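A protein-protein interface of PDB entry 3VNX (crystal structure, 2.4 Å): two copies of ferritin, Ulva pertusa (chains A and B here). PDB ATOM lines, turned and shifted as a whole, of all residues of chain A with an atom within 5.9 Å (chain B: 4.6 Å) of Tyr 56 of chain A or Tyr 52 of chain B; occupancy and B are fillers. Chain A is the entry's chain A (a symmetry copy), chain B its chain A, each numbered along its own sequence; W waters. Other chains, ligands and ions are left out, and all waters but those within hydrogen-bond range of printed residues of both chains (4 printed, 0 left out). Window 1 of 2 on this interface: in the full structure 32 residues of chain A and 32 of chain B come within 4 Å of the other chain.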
ATOM      1  N   GLU A  51      -7.668  32.600 -29.072  1.00  0.00           N
ATOM      2  CA  GLU A  51      -7.860  31.612 -30.129  1.00  0.00           C
ATOM      3  C   GLU A  51      -8.841  30.584 -29.618  1.00  0.00           C
ATOM      4  O   GLU A  51      -9.797  30.193 -30.317  1.00  0.00           O
ATOM      5  CB  GLU A  51      -6.541  30.916 -30.506  1.00  0.00           C
ATOM      6  CG  GLU A  51      -5.413  31.837 -30.976  1.00  0.00           C
ATOM      7  CD  GLU A  51      -5.602  32.415 -32.393  1.00  0.00           C
ATOM      8  OE1 GLU A  51      -4.806  33.308 -32.768  1.00  0.00           O
ATOM      9  OE2 GLU A  51      -6.519  31.992 -33.137  1.00  0.00           O
ATOM     10  N   TYR A  52      -8.609  30.152 -28.385  1.00  0.00           N
ATOM     11  CA  TYR A  52      -9.502  29.174 -27.776  1.00  0.00           C
ATOM     12  C   TYR A  52     -10.947  29.683 -27.725  1.00  0.00           C
ATOM     13  O   TYR A  52     -11.867  28.923 -28.019  1.00  0.00           O
ATOM     14  CB  TYR A  52      -9.005  28.728 -26.398  1.00  0.00           C
ATOM     15  CG  TYR A  52      -8.859  27.221 -26.264  1.00  0.00           C
ATOM     16  CD1 TYR A  52      -9.929  26.376 -26.553  1.00  0.00           C
ATOM     17  CD2 TYR A  52      -7.655  26.643 -25.847  1.00  0.00           C
ATOM     18  CE1 TYR A  52      -9.810  24.991 -26.442  1.00  0.00           C
ATOM     19  CE2 TYR A  52      -7.522  25.254 -25.717  1.00  0.00           C
ATOM     20  CZ  TYR A  52      -8.609  24.432 -26.020  1.00  0.00           C
ATOM     21  OH  TYR A  52      -8.513  23.052 -25.901  1.00  0.00           O
ATOM     22  N   THR A  53     -11.154  30.958 -27.395  1.00  0.00           N
ATOM     23  CA  THR A  53     -12.503  31.535 -27.378  1.00  0.00           C
ATOM     24  C   THR A  53     -13.116  31.536 -28.774  1.00  0.00           C
ATOM     25  O   THR A  53     -14.267  31.122 -28.969  1.00  0.00           O
ATOM     26  CB  THR A  53     -12.525  32.992 -26.842  1.00  0.00           C
ATOM     27  OG1 THR A  53     -12.199  32.999 -25.451  1.00  0.00           O
ATOM     28  CG2 THR A  53     -13.902  33.609 -27.023  1.00  0.00           C
ATOM     29  N   ILE A  54     -12.340  32.010 -29.747  1.00  0.00           N
ATOM     30  CA  ILE A  54     -12.821  32.089 -31.131  1.00  0.00           C
ATOM     31  C   ILE A  54     -13.153  30.700 -31.712  1.00  0.00           C
ATOM     32  O   ILE A  54     -14.100  30.534 -32.485  1.00  0.00           O
ATOM     33  CB  ILE A  54     -11.810  32.821 -32.018  1.00  0.00           C
ATOM     34  CG1 ILE A  54     -11.733  34.295 -31.613  1.00  0.00           C
ATOM     35  CG2 ILE A  54     -12.168  32.677 -33.484  1.00  0.00           C
ATOM     36  CD1 ILE A  54     -10.644  35.042 -32.337  1.00  0.00           C
ATOM     37  N   SER A  55     -12.370  29.704 -31.324  1.00  0.00           N
ATOM     38  CA  SER A  55     -12.680  28.338 -31.697  1.00  0.00           C
ATOM     39  C   SER A  55     -14.073  27.955 -31.189  1.00  0.00           C
ATOM     40  O   SER A  55     -14.854  27.323 -31.904  1.00  0.00           O
ATOM     41  CB  SER A  55     -11.626  27.391 -31.132  1.00  0.00           C
ATOM     42  OG  SER A  55     -12.037  26.057 -31.289  1.00  0.00           O
ATOM     43  N   TYR A  56     -14.381  28.353 -29.954  1.00  0.00           N
ATOM     44  CA  TYR A  56     -15.640  27.977 -29.307  1.00  0.00           C
ATOM     45  C   TYR A  56     -16.807  28.693 -29.998  1.00  0.00           C
ATOM     46  O   TYR A  56     -17.864  28.106 -30.262  1.00  0.00           O
ATOM     47  CB  TYR A  56     -15.565  28.362 -27.833  1.00  0.00           C
ATOM     48  CG  TYR A  56     -16.426  27.573 -26.852  1.00  0.00           C
ATOM     49  CD1 TYR A  56     -16.429  26.186 -26.844  1.00  0.00           C
ATOM     50  CD2 TYR A  56     -17.186  28.237 -25.888  1.00  0.00           C
ATOM     51  CE1 TYR A  56     -17.195  25.477 -25.913  1.00  0.00           C
ATOM     52  CE2 TYR A  56     -17.956  27.546 -24.962  1.00  0.00           C
ATOM     53  CZ  TYR A  56     -17.955  26.170 -24.970  1.00  0.00           C
ATOM     54  OH  TYR A  56     -18.722  25.487 -24.045  1.00  0.00           O
ATOM     55  N   VAL A  57     -16.598  29.967 -30.297  1.00  0.00           N
ATOM     56  CA  VAL A  57     -17.586  30.751 -31.018  1.00  0.00           C
ATOM     57  C   VAL A  57     -17.854  30.130 -32.373  1.00  0.00           C
ATOM     58  O   VAL A  57     -19.009  29.992 -32.784  1.00  0.00           O
ATOM     59  CB  VAL A  57     -17.093  32.173 -31.244  1.00  0.00           C
ATOM     60  CG1 VAL A  57     -18.059  32.918 -32.146  1.00  0.00           C
ATOM     61  CG2 VAL A  57     -16.914  32.882 -29.913  1.00  0.00           C
ATOM     62  N   TYR A  58     -16.786  29.758 -33.076  1.00  0.00           N
ATOM     63  CA  TYR A  58     -16.956  29.123 -34.376  1.00  0.00           C
ATOM     64  C   TYR A  58     -17.735  27.821 -34.269  1.00  0.00           C
ATOM     65  O   TYR A  58     -18.524  27.484 -35.160  1.00  0.00           O
ATOM     66  CB  TYR A  58     -15.618  28.909 -35.078  1.00  0.00           C
ATOM     67  CG  TYR A  58     -15.131  30.179 -35.741  1.00  0.00           C
ATOM     68  CD1 TYR A  58     -16.034  31.172 -36.099  1.00  0.00           C
ATOM     69  CD2 TYR A  58     -13.782  30.393 -36.003  1.00  0.00           C
ATOM     70  CE1 TYR A  58     -15.615  32.344 -36.701  1.00  0.00           C
ATOM     71  CE2 TYR A  58     -13.349  31.570 -36.608  1.00  0.00           C
ATOM     72  CZ  TYR A  58     -14.277  32.548 -36.958  1.00  0.00           C
ATOM     73  OH  TYR A  58     -13.883  33.736 -37.559  1.00  0.00           O
ATOM     74  N   HIS A  59     -17.526  27.100 -33.168  1.00  0.00           N
ATOM     75  CA  HIS A  59     -18.249  25.862 -32.950  1.00  0.00           C
ATOM     76  C   HIS A  59     -19.742  26.153 -32.758  1.00  0.00           C
ATOM     77  O   HIS A  59     -20.601  25.391 -33.219  1.00  0.00           O
ATOM     78  CB  HIS A  59     -17.684  25.093 -31.759  1.00  0.00           C
ATOM     79  CG  HIS A  59     -17.861  23.615 -31.876  1.00  0.00           C
ATOM     80  ND1 HIS A  59     -17.273  22.721 -31.002  1.00  0.00           N
ATOM     81  CD2 HIS A  59     -18.542  22.865 -32.774  1.00  0.00           C
ATOM     82  CE1 HIS A  59     -17.597  21.489 -31.354  1.00  0.00           C
ATOM     83  NE2 HIS A  59     -18.372  21.549 -32.425  1.00  0.00           N
ATOM     84  N   ALA A  60     -20.052  27.265 -32.094  1.00  0.00           N
ATOM     85  CA  ALA A  60     -21.455  27.651 -31.924  1.00  0.00           C
ATOM     86  C   ALA A  60     -22.099  27.982 -33.286  1.00  0.00           C
ATOM     87  O   ALA A  60     -23.245  27.588 -33.567  1.00  0.00           O
ATOM     88  CB  ALA A  60     -21.586  28.817 -30.941  1.00  0.00           C
ATOM     89  N   LEU A  61     -21.348  28.678 -34.139  1.00  0.00           N
ATOM     90  CA  LEU A  61     -21.837  29.018 -35.465  1.00  0.00           C
ATOM     91  C   LEU A  61     -22.157  27.757 -36.237  1.00  0.00           C
ATOM     92  O   LEU A  61     -23.165  27.668 -36.952  1.00  0.00           O
ATOM     93  CB  LEU A  61     -20.796  29.838 -36.211  1.00  0.00           C
ATOM     94  CG  LEU A  61     -20.861  31.311 -35.805  1.00  0.00           C
ATOM     95  CD1 LEU A  61     -19.592  32.070 -36.210  1.00  0.00           C
ATOM     96  CD2 LEU A  61     -22.105  31.945 -36.410  1.00  0.00           C
ATOM     97  N   SER A  83     -13.407  26.074 -36.487  1.00  0.00           N
ATOM     98  CA  SER A  83     -13.275  25.804 -35.056  1.00  0.00           C
ATOM     99  C   SER A  83     -12.079  24.893 -34.733  1.00  0.00           C
ATOM    100  O   SER A  83     -11.271  25.203 -33.850  1.00  0.00           O
ATOM    101  CB  SER A  83     -14.564  25.245 -34.456  1.00  0.00           C
ATOM    102  OG  SER A  83     -14.342  24.904 -33.097  1.00  0.00           O
ATOM    103  N   LEU A 109     -13.703  30.165 -20.527  1.00  0.00           N
ATOM    104  CA  LEU A 109     -14.333  30.473 -21.795  1.00  0.00           C
ATOM    105  C   LEU A 109     -15.770  30.865 -21.527  1.00  0.00           C
ATOM    106  O   LEU A 109     -16.531  30.085 -20.934  1.00  0.00           O
ATOM    107  CB  LEU A 109     -14.293  29.266 -22.731  1.00  0.00           C
ATOM    108  CG  LEU A 109     -12.925  28.687 -23.117  1.00  0.00           C
ATOM    109  CD1 LEU A 109     -13.078  27.839 -24.370  1.00  0.00           C
ATOM    110  CD2 LEU A 109     -11.898  29.785 -23.346  1.00  0.00           C
ATOM    111  N   ALA A 110     -16.135  32.079 -21.940  1.00  0.00           N
ATOM    112  CA  ALA A 110     -17.515  32.538 -21.838  1.00  0.00           C
ATOM    113  C   ALA A 110     -18.423  31.787 -22.818  1.00  0.00           C
ATOM    114  O   ALA A 110     -17.985  31.370 -23.899  1.00  0.00           O
ATOM    115  CB  ALA A 110     -17.591  34.039 -22.092  1.00  0.00           C
ATOM    116  N   ALA A 111     -19.688  31.624 -22.439  1.00  0.00           N
ATOM    117  CA  ALA A 111     -20.694  31.067 -23.338  1.00  0.00           C
ATOM    118  C   ALA A 111     -20.794  31.943 -24.567  1.00  0.00           C
ATOM    119  O   ALA A 111     -20.945  33.161 -24.441  1.00  0.00           O
ATOM    120  CB  ALA A 111     -22.021  31.013 -22.648  1.00  0.00           C
ATOM    121  N   PRO A 112     -20.699  31.337 -25.768  1.00  0.00           N
ATOM    122  CA  PRO A 112     -20.822  32.096 -27.024  1.00  0.00           C
ATOM    123  C   PRO A 112     -22.281  32.333 -27.362  1.00  0.00           C
ATOM    124  O   PRO A 112     -23.149  31.669 -26.796  1.00  0.00           O
ATOM    125  CB  PRO A 112     -20.222  31.150 -28.060  1.00  0.00           C
ATOM    126  CG  PRO A 112     -20.524  29.776 -27.510  1.00  0.00           C
ATOM    127  CD  PRO A 112     -20.427  29.904 -26.007  1.00  0.00           C
ATOM    128  N   ILE B  48     -22.963  17.809 -23.176  1.00  0.00           N
ATOM    129  CA  ILE B  48     -22.032  18.506 -24.054  1.00  0.00           C
ATOM    130  C   ILE B  48     -21.023  19.304 -23.223  1.00  0.00           C
ATOM    131  O   ILE B  48     -19.802  19.179 -23.415  1.00  0.00           O
ATOM    132  CB  ILE B  48     -22.748  19.432 -25.050  1.00  0.00           C
ATOM    133  CG1 ILE B  48     -23.384  18.607 -26.162  1.00  0.00           C
ATOM    134  CG2 ILE B  48     -21.767  20.424 -25.655  1.00  0.00           C
ATOM    135  CD1 ILE B  48     -24.573  19.257 -26.816  1.00  0.00           C
ATOM    136  N   ASN B  49     -21.524  20.106 -22.287  1.00  0.00           N
ATOM    137  CA  ASN B  49     -20.640  20.944 -21.484  1.00  0.00           C
ATOM    138  C   ASN B  49     -19.664  20.124 -20.654  1.00  0.00           C
ATOM    139  O   ASN B  49     -18.537  20.553 -20.403  1.00  0.00           O
ATOM    140  CB  ASN B  49     -21.444  21.891 -20.578  1.00  0.00           C
ATOM    141  CG  ASN B  49     -20.549  22.753 -19.679  1.00  0.00           C
ATOM    142  OD1 ASN B  49     -20.548  22.599 -18.453  1.00  0.00           O
ATOM    143  ND2 ASN B  49     -19.781  23.659 -20.289  1.00  0.00           N
ATOM    144  N   ILE B  50     -20.099  18.941 -20.228  1.00  0.00           N
ATOM    145  CA  ILE B  50     -19.257  18.071 -19.411  1.00  0.00           C
ATOM    146  C   ILE B  50     -18.079  17.505 -20.223  1.00  0.00           C
ATOM    147  O   ILE B  50     -16.942  17.441 -19.737  1.00  0.00           O
ATOM    148  CB  ILE B  50     -20.097  16.946 -18.779  1.00  0.00           C
ATOM    149  CG1 ILE B  50     -21.159  17.555 -17.861  1.00  0.00           C
ATOM    150  CG2 ILE B  50     -19.211  15.954 -18.020  1.00  0.00           C
ATOM    151  CD1 ILE B  50     -21.912  16.559 -17.030  1.00  0.00           C
ATOM    152  N   GLU B  51     -18.354  17.109 -21.468  1.00  0.00           N
ATOM    153  CA  GLU B  51     -17.319  16.567 -22.343  1.00  0.00           C
ATOM    154  C   GLU B  51     -16.398  17.703 -22.716  1.00  0.00           C
ATOM    155  O   GLU B  51     -15.158  17.579 -22.667  1.00  0.00           O
ATOM    156  CB  GLU B  51     -17.916  15.952 -23.620  1.00  0.00           C
ATOM    157  CG  GLU B  51     -18.932  14.828 -23.406  1.00  0.00           C
ATOM    158  CD  GLU B  51     -18.322  13.487 -22.954  1.00  0.00           C
ATOM    159  OE1 GLU B  51     -19.111  12.580 -22.596  1.00  0.00           O
ATOM    160  OE2 GLU B  51     -17.080  13.318 -22.957  1.00  0.00           O
ATOM    161  N   TYR B  52     -17.010  18.824 -23.080  1.00  0.00           N
ATOM    162  CA  TYR B  52     -16.225  19.997 -23.442  1.00  0.00           C
ATOM    163  C   TYR B  52     -15.300  20.433 -22.300  1.00  0.00           C
ATOM    164  O   TYR B  52     -14.143  20.763 -22.550  1.00  0.00           O
ATOM    165  CB  TYR B  52     -17.109  21.147 -23.932  1.00  0.00           C
ATOM    166  CG  TYR B  52     -16.716  21.676 -25.301  1.00  0.00           C
ATOM    167  CD1 TYR B  52     -15.410  22.093 -25.552  1.00  0.00           C
ATOM    168  CD2 TYR B  52     -17.648  21.761 -26.341  1.00  0.00           C
ATOM    169  CE1 TYR B  52     -15.030  22.573 -26.806  1.00  0.00           C
ATOM    170  CE2 TYR B  52     -17.287  22.254 -27.602  1.00  0.00           C
ATOM    171  CZ  TYR B  52     -15.970  22.658 -27.827  1.00  0.00           C
ATOM    172  OH  TYR B  52     -15.578  23.152 -29.064  1.00  0.00           O
ATOM    173  N   THR B  53     -15.780  20.404 -21.056  1.00  0.00           N
ATOM    174  CA  THR B  53     -14.940  20.754 -19.904  1.00  0.00           C
ATOM    175  C   THR B  53     -13.786  19.770 -19.749  1.00  0.00           C
ATOM    176  O   THR B  53     -12.625  20.166 -19.576  1.00  0.00           O
ATOM    177  CB  THR B  53     -15.735  20.778 -18.570  1.00  0.00           C
ATOM    178  OG1 THR B  53     -16.663  21.864 -18.580  1.00  0.00           O
ATOM    179  CG2 THR B  53     -14.794  20.952 -17.389  1.00  0.00           C
ATOM    180  N   ILE B  54     -14.113  18.479 -19.806  1.00  0.00           N
ATOM    181  CA  ILE B  54     -13.098  17.432 -19.645  1.00  0.00           C
ATOM    182  C   ILE B  54     -12.029  17.483 -20.755  1.00  0.00           C
ATOM    183  O   ILE B  54     -10.845  17.221 -20.522  1.00  0.00           O
ATOM    184  CB  ILE B  54     -13.750  16.048 -19.582  1.00  0.00           C
ATOM    185  CG1 ILE B  54     -14.565  15.915 -18.294  1.00  0.00           C
ATOM    186  CG2 ILE B  54     -12.708  14.951 -19.682  1.00  0.00           C
ATOM    187  CD1 ILE B  54     -15.363  14.638 -18.238  1.00  0.00           C
ATOM    188  N   SER B  55     -12.455  17.832 -21.959  1.00  0.00           N
ATOM    189  CA  SER B  55     -11.511  18.048 -23.038  1.00  0.00           C
ATOM    190  C   SER B  55     -10.509  19.139 -22.652  1.00  0.00           C
ATOM    191  O   SER B  55      -9.308  19.009 -22.900  1.00  0.00           O
ATOM    192  CB  SER B  55     -12.256  18.433 -24.313  1.00  0.00           C
ATOM    193  OG  SER B  55     -11.348  18.866 -25.294  1.00  0.00           O
ATOM    194  N   TYR B  56     -11.009  20.210 -22.033  1.00  0.00           N
ATOM    195  CA  TYR B  56     -10.182  21.368 -21.691  1.00  0.00           C
ATOM    196  C   TYR B  56      -9.200  20.988 -20.577  1.00  0.00           C
ATOM    197  O   TYR B  56      -8.014  21.341 -20.607  1.00  0.00           O
ATOM    198  CB  TYR B  56     -11.095  22.505 -21.244  1.00  0.00           C
ATOM    199  CG  TYR B  56     -10.586  23.932 -21.419  1.00  0.00           C
ATOM    200  CD1 TYR B  56     -10.060  24.370 -22.626  1.00  0.00           C
ATOM    201  CD2 TYR B  56     -10.701  24.855 -20.380  1.00  0.00           C
ATOM    202  CE1 TYR B  56      -9.632  25.692 -22.782  1.00  0.00           C
ATOM    203  CE2 TYR B  56     -10.274  26.169 -20.519  1.00  0.00           C
ATOM    204  CZ  TYR B  56      -9.748  26.588 -21.719  1.00  0.00           C
ATOM    205  OH  TYR B  56      -9.326  27.897 -21.853  1.00  0.00           O
ATOM    206  N   ARG B  87     -13.466  16.296 -26.984  1.00  0.00           N
ATOM    207  CA  ARG B  87     -14.072  17.395 -27.733  1.00  0.00           C
ATOM    208  C   ARG B  87     -14.943  16.838 -28.844  1.00  0.00           C
ATOM    209  O   ARG B  87     -16.007  17.378 -29.140  1.00  0.00           O
ATOM    210  CB  ARG B  87     -12.998  18.319 -28.312  1.00  0.00           C
ATOM    211  CG  ARG B  87     -13.536  19.386 -29.235  1.00  0.00           C
ATOM    212  CD  ARG B  87     -12.491  20.468 -29.485  1.00  0.00           C
ATOM    213  NE  ARG B  87     -12.888  21.422 -30.525  1.00  0.00           N
ATOM    214  CZ  ARG B  87     -12.749  21.218 -31.834  1.00  0.00           C
ATOM    215  NH1 ARG B  87     -12.230  20.070 -32.285  1.00  0.00           N
ATOM    216  NH2 ARG B  87     -13.128  22.161 -32.698  1.00  0.00           N
ATOM    217  N   ALA B  90     -18.173  15.754 -27.392  1.00  0.00           N
ATOM    218  CA  ALA B  90     -19.056  16.917 -27.332  1.00  0.00           C
ATOM    219  C   ALA B  90     -19.697  17.188 -28.691  1.00  0.00           C
ATOM    220  O   ALA B  90     -20.913  17.412 -28.791  1.00  0.00           O
ATOM    221  CB  ALA B  90     -18.299  18.148 -26.836  1.00  0.00           C
ATOM    222  N   MET B  94     -23.643  17.301 -29.880  1.00  0.00           N
ATOM    223  CA  MET B  94     -24.206  18.459 -30.565  1.00  0.00           C
ATOM    224  C   MET B  94     -24.879  18.016 -31.850  1.00  0.00           C
ATOM    225  O   MET B  94     -25.985  18.463 -32.187  1.00  0.00           O
ATOM    226  CB  MET B  94     -23.112  19.494 -30.835  1.00  0.00           C
ATOM    227  CG  MET B  94     -22.415  19.947 -29.551  1.00  0.00           C
ATOM    228  SD  MET B  94     -20.861  20.822 -29.784  1.00  0.00           S
ATOM    229  CE  MET B  94     -21.424  22.263 -30.710  1.00  0.00           C
ATOM    230  N   LEU B 106     -24.105  26.220 -25.729  1.00  0.00           N
ATOM    231  CA  LEU B 106     -22.752  26.059 -25.226  1.00  0.00           C
ATOM    232  C   LEU B 106     -22.584  26.921 -23.991  1.00  0.00           C
ATOM    233  O   LEU B 106     -22.943  28.101 -23.981  1.00  0.00           O
ATOM    234  CB  LEU B 106     -21.713  26.436 -26.292  1.00  0.00           C
ATOM    235  CG  LEU B 106     -21.440  25.388 -27.372  1.00  0.00           C
ATOM    236  CD1 LEU B 106     -20.359  25.862 -28.330  1.00  0.00           C
ATOM    237  CD2 LEU B 106     -21.054  24.058 -26.727  1.00  0.00           C
ATOM    238  N   LYS B 107     -22.021  26.321 -22.955  1.00  0.00           N
ATOM    239  CA  LYS B 107     -21.936  26.954 -21.653  1.00  0.00           C
ATOM    240  C   LYS B 107     -20.509  27.407 -21.349  1.00  0.00           C
ATOM    241  O   LYS B 107     -19.587  27.126 -22.110  1.00  0.00           O
ATOM    242  CB  LYS B 107     -22.448  25.979 -20.602  1.00  0.00           C
ATOM    243  CG  LYS B 107     -23.886  25.548 -20.852  1.00  0.00           C
ATOM    244  CD  LYS B 107     -24.352  24.540 -19.806  1.00  0.00           C
ATOM    245  CE  LYS B 107     -25.875  24.518 -19.688  1.00  0.00           C
ATOM    246  NZ  LYS B 107     -26.338  23.447 -18.755  1.00  0.00           N
ATOM    247  N   LEU B 109     -16.761  27.604 -19.834  1.00  0.00           N
ATOM    248  CA  LEU B 109     -15.771  26.643 -19.390  1.00  0.00           C
ATOM    249  C   LEU B 109     -14.913  27.303 -18.332  1.00  0.00           C
ATOM    250  O   LEU B 109     -14.299  28.350 -18.586  1.00  0.00           O
ATOM    251  CB  LEU B 109     -14.894  26.187 -20.555  1.00  0.00           C
ATOM    252  CG  LEU B 109     -15.570  25.510 -21.755  1.00  0.00           C
ATOM    253  CD1 LEU B 109     -14.525  24.739 -22.546  1.00  0.00           C
ATOM    254  CD2 LEU B 109     -16.690  24.579 -21.314  1.00  0.00           C
HETATM  255  O   HOH W   1     -10.319  21.165 -26.372  1.00  0.00           O
HETATM  256  O   HOH W   2     -20.658  23.661 -23.079  1.00  0.00           O
HETATM  257  O   HOH W   3     -24.536  30.297 -24.955  1.00  0.00           O
HETATM  258  O   HOH W   4     -13.207  24.014 -29.889  1.00  0.00           O
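The side-chain hydroxyl (OH) of Tyr 52 of chain B is in hydrogen-bond range of a ring nitrogen (ND1) of His 59 of chain A (2.6 Å).
The guanidinium group (NH2) of Arg 87 of chain B is in hydrogen-bond range of the side-chain hydroxyl (OG) of Ser 83 of chain A, at 3.0 Å.
The side-chain sulfur of Met 94 of chain B sits close to a ring nitrogen (NE2) of His 59 of chain A (3.7 Å).
The backbone carbonyl oxygen of Lys 107 of chain B is in hydrogen-bond range of the side-chain hydroxyl of Tyr 56 of chain A.
N of Leu 109 of chain B is in hydrogen-bond range of O of Leu 109 of chain A (2.7 Å).
The backbone carbonyl oxygen (O) of Ser 55 of chain A sits at hydrogen-bond distance from the side-chain hydroxyl (OG) of Ser 83 of chain A (2.7 Å).
CZ of Tyr 52 of chain A touches CE1 of Tyr 56 of chain B, at 3.6 Å.
CZ of Tyr 52 of chain B touches CE1 of Tyr 56 of chain A, 3.6 Å away.
OH of Tyr 56 of chain A touches CD2 of Leu 106 of chain B, 3.8 Å away.
Tyr 56 of chain A touches Leu 109 of chain B (OH to CD2, 3.5 Å).
Leu 109 of chain A touches Tyr 56 of chain B.
O of Leu 106 of chain B touches CB of Ala 111 of chain A (3.3 Å).
O of Leu 106 of chain B touches CD of Pro 112 of chain A, 3.7 Å away.
Tyr 56 of chain A touches four residues of chain B.
Of the printed residues of chain B, Ser 83 of chain A touches Arg 87 (3.0 Å).
Ala 90 of chain B touches none of the printed residues of chain A.
Of the printed residues of chain A, Lys 107 of chain B touches Tyr 56 (2.7 Å).
The nearest residue of chain B that does not touch Tyr 56 of chain A is Asn 49 of chain B (4.3 Å).
The nearest residue of chain A that does not touch Tyr 52 of chain B is Ser 83 of chain A (4.6 Å).
The nearest printed residue of chain B that does not touch Pro 112 of chain A is Lys 107 of chain B (4.9 Å).
Hydrophobic or aromatic side chains of chain A that line the printed part of chain B: Tyr 52, Tyr 56, His 59, Leu 109, Ala 111 and Pro 112.
Among the printed residues, 12 pairs touch across the chains.
Tyr 52 of chain A touches Tyr 56 of chain B, and with the chains exchanged Tyr 56 of chain A touches Tyr 52 of chain B.
Tyr 56 of chain A touches Leu 109 of chain B, and with the chains exchanged Leu 109 of chain A touches Tyr 56 of chain B.
Leu 109 of chain A touches its own counterpart, Leu 109 of chain B.
Of the 12 pairs that touch across the chains among the printed residues, 5 have their exchanged pair printed and touching as well.
Water W1 bridges OH of Tyr 52 of chain A (2.7 Å) and OG of Ser 55 of chain B (2.7 Å).
Water W4 lies within hydrogen-bond range of the side-chain hydroxyl of Tyr 52 of chain B, the guanidinium group of Arg 87 of chain B and the side-chain hydroxyl of Ser 55 of chain A.
Water W3 bridges the backbone carbonyl oxygen (O) of Pro 112 of chain A (2.7 Å) and the backbone carbonyl oxygen (O) of Leu 106 of chain B (2.9 Å).
Water W2 lies within hydrogen-bond range of the side-chain hydroxyl (OH) of Tyr 56 of chain A (2.8 Å), the side-chain amide nitrogen (ND2) of Asn 49 of chain B (2.9 Å) and the backbone NH (N) of Lys 107 of chain B (3.0 Å).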
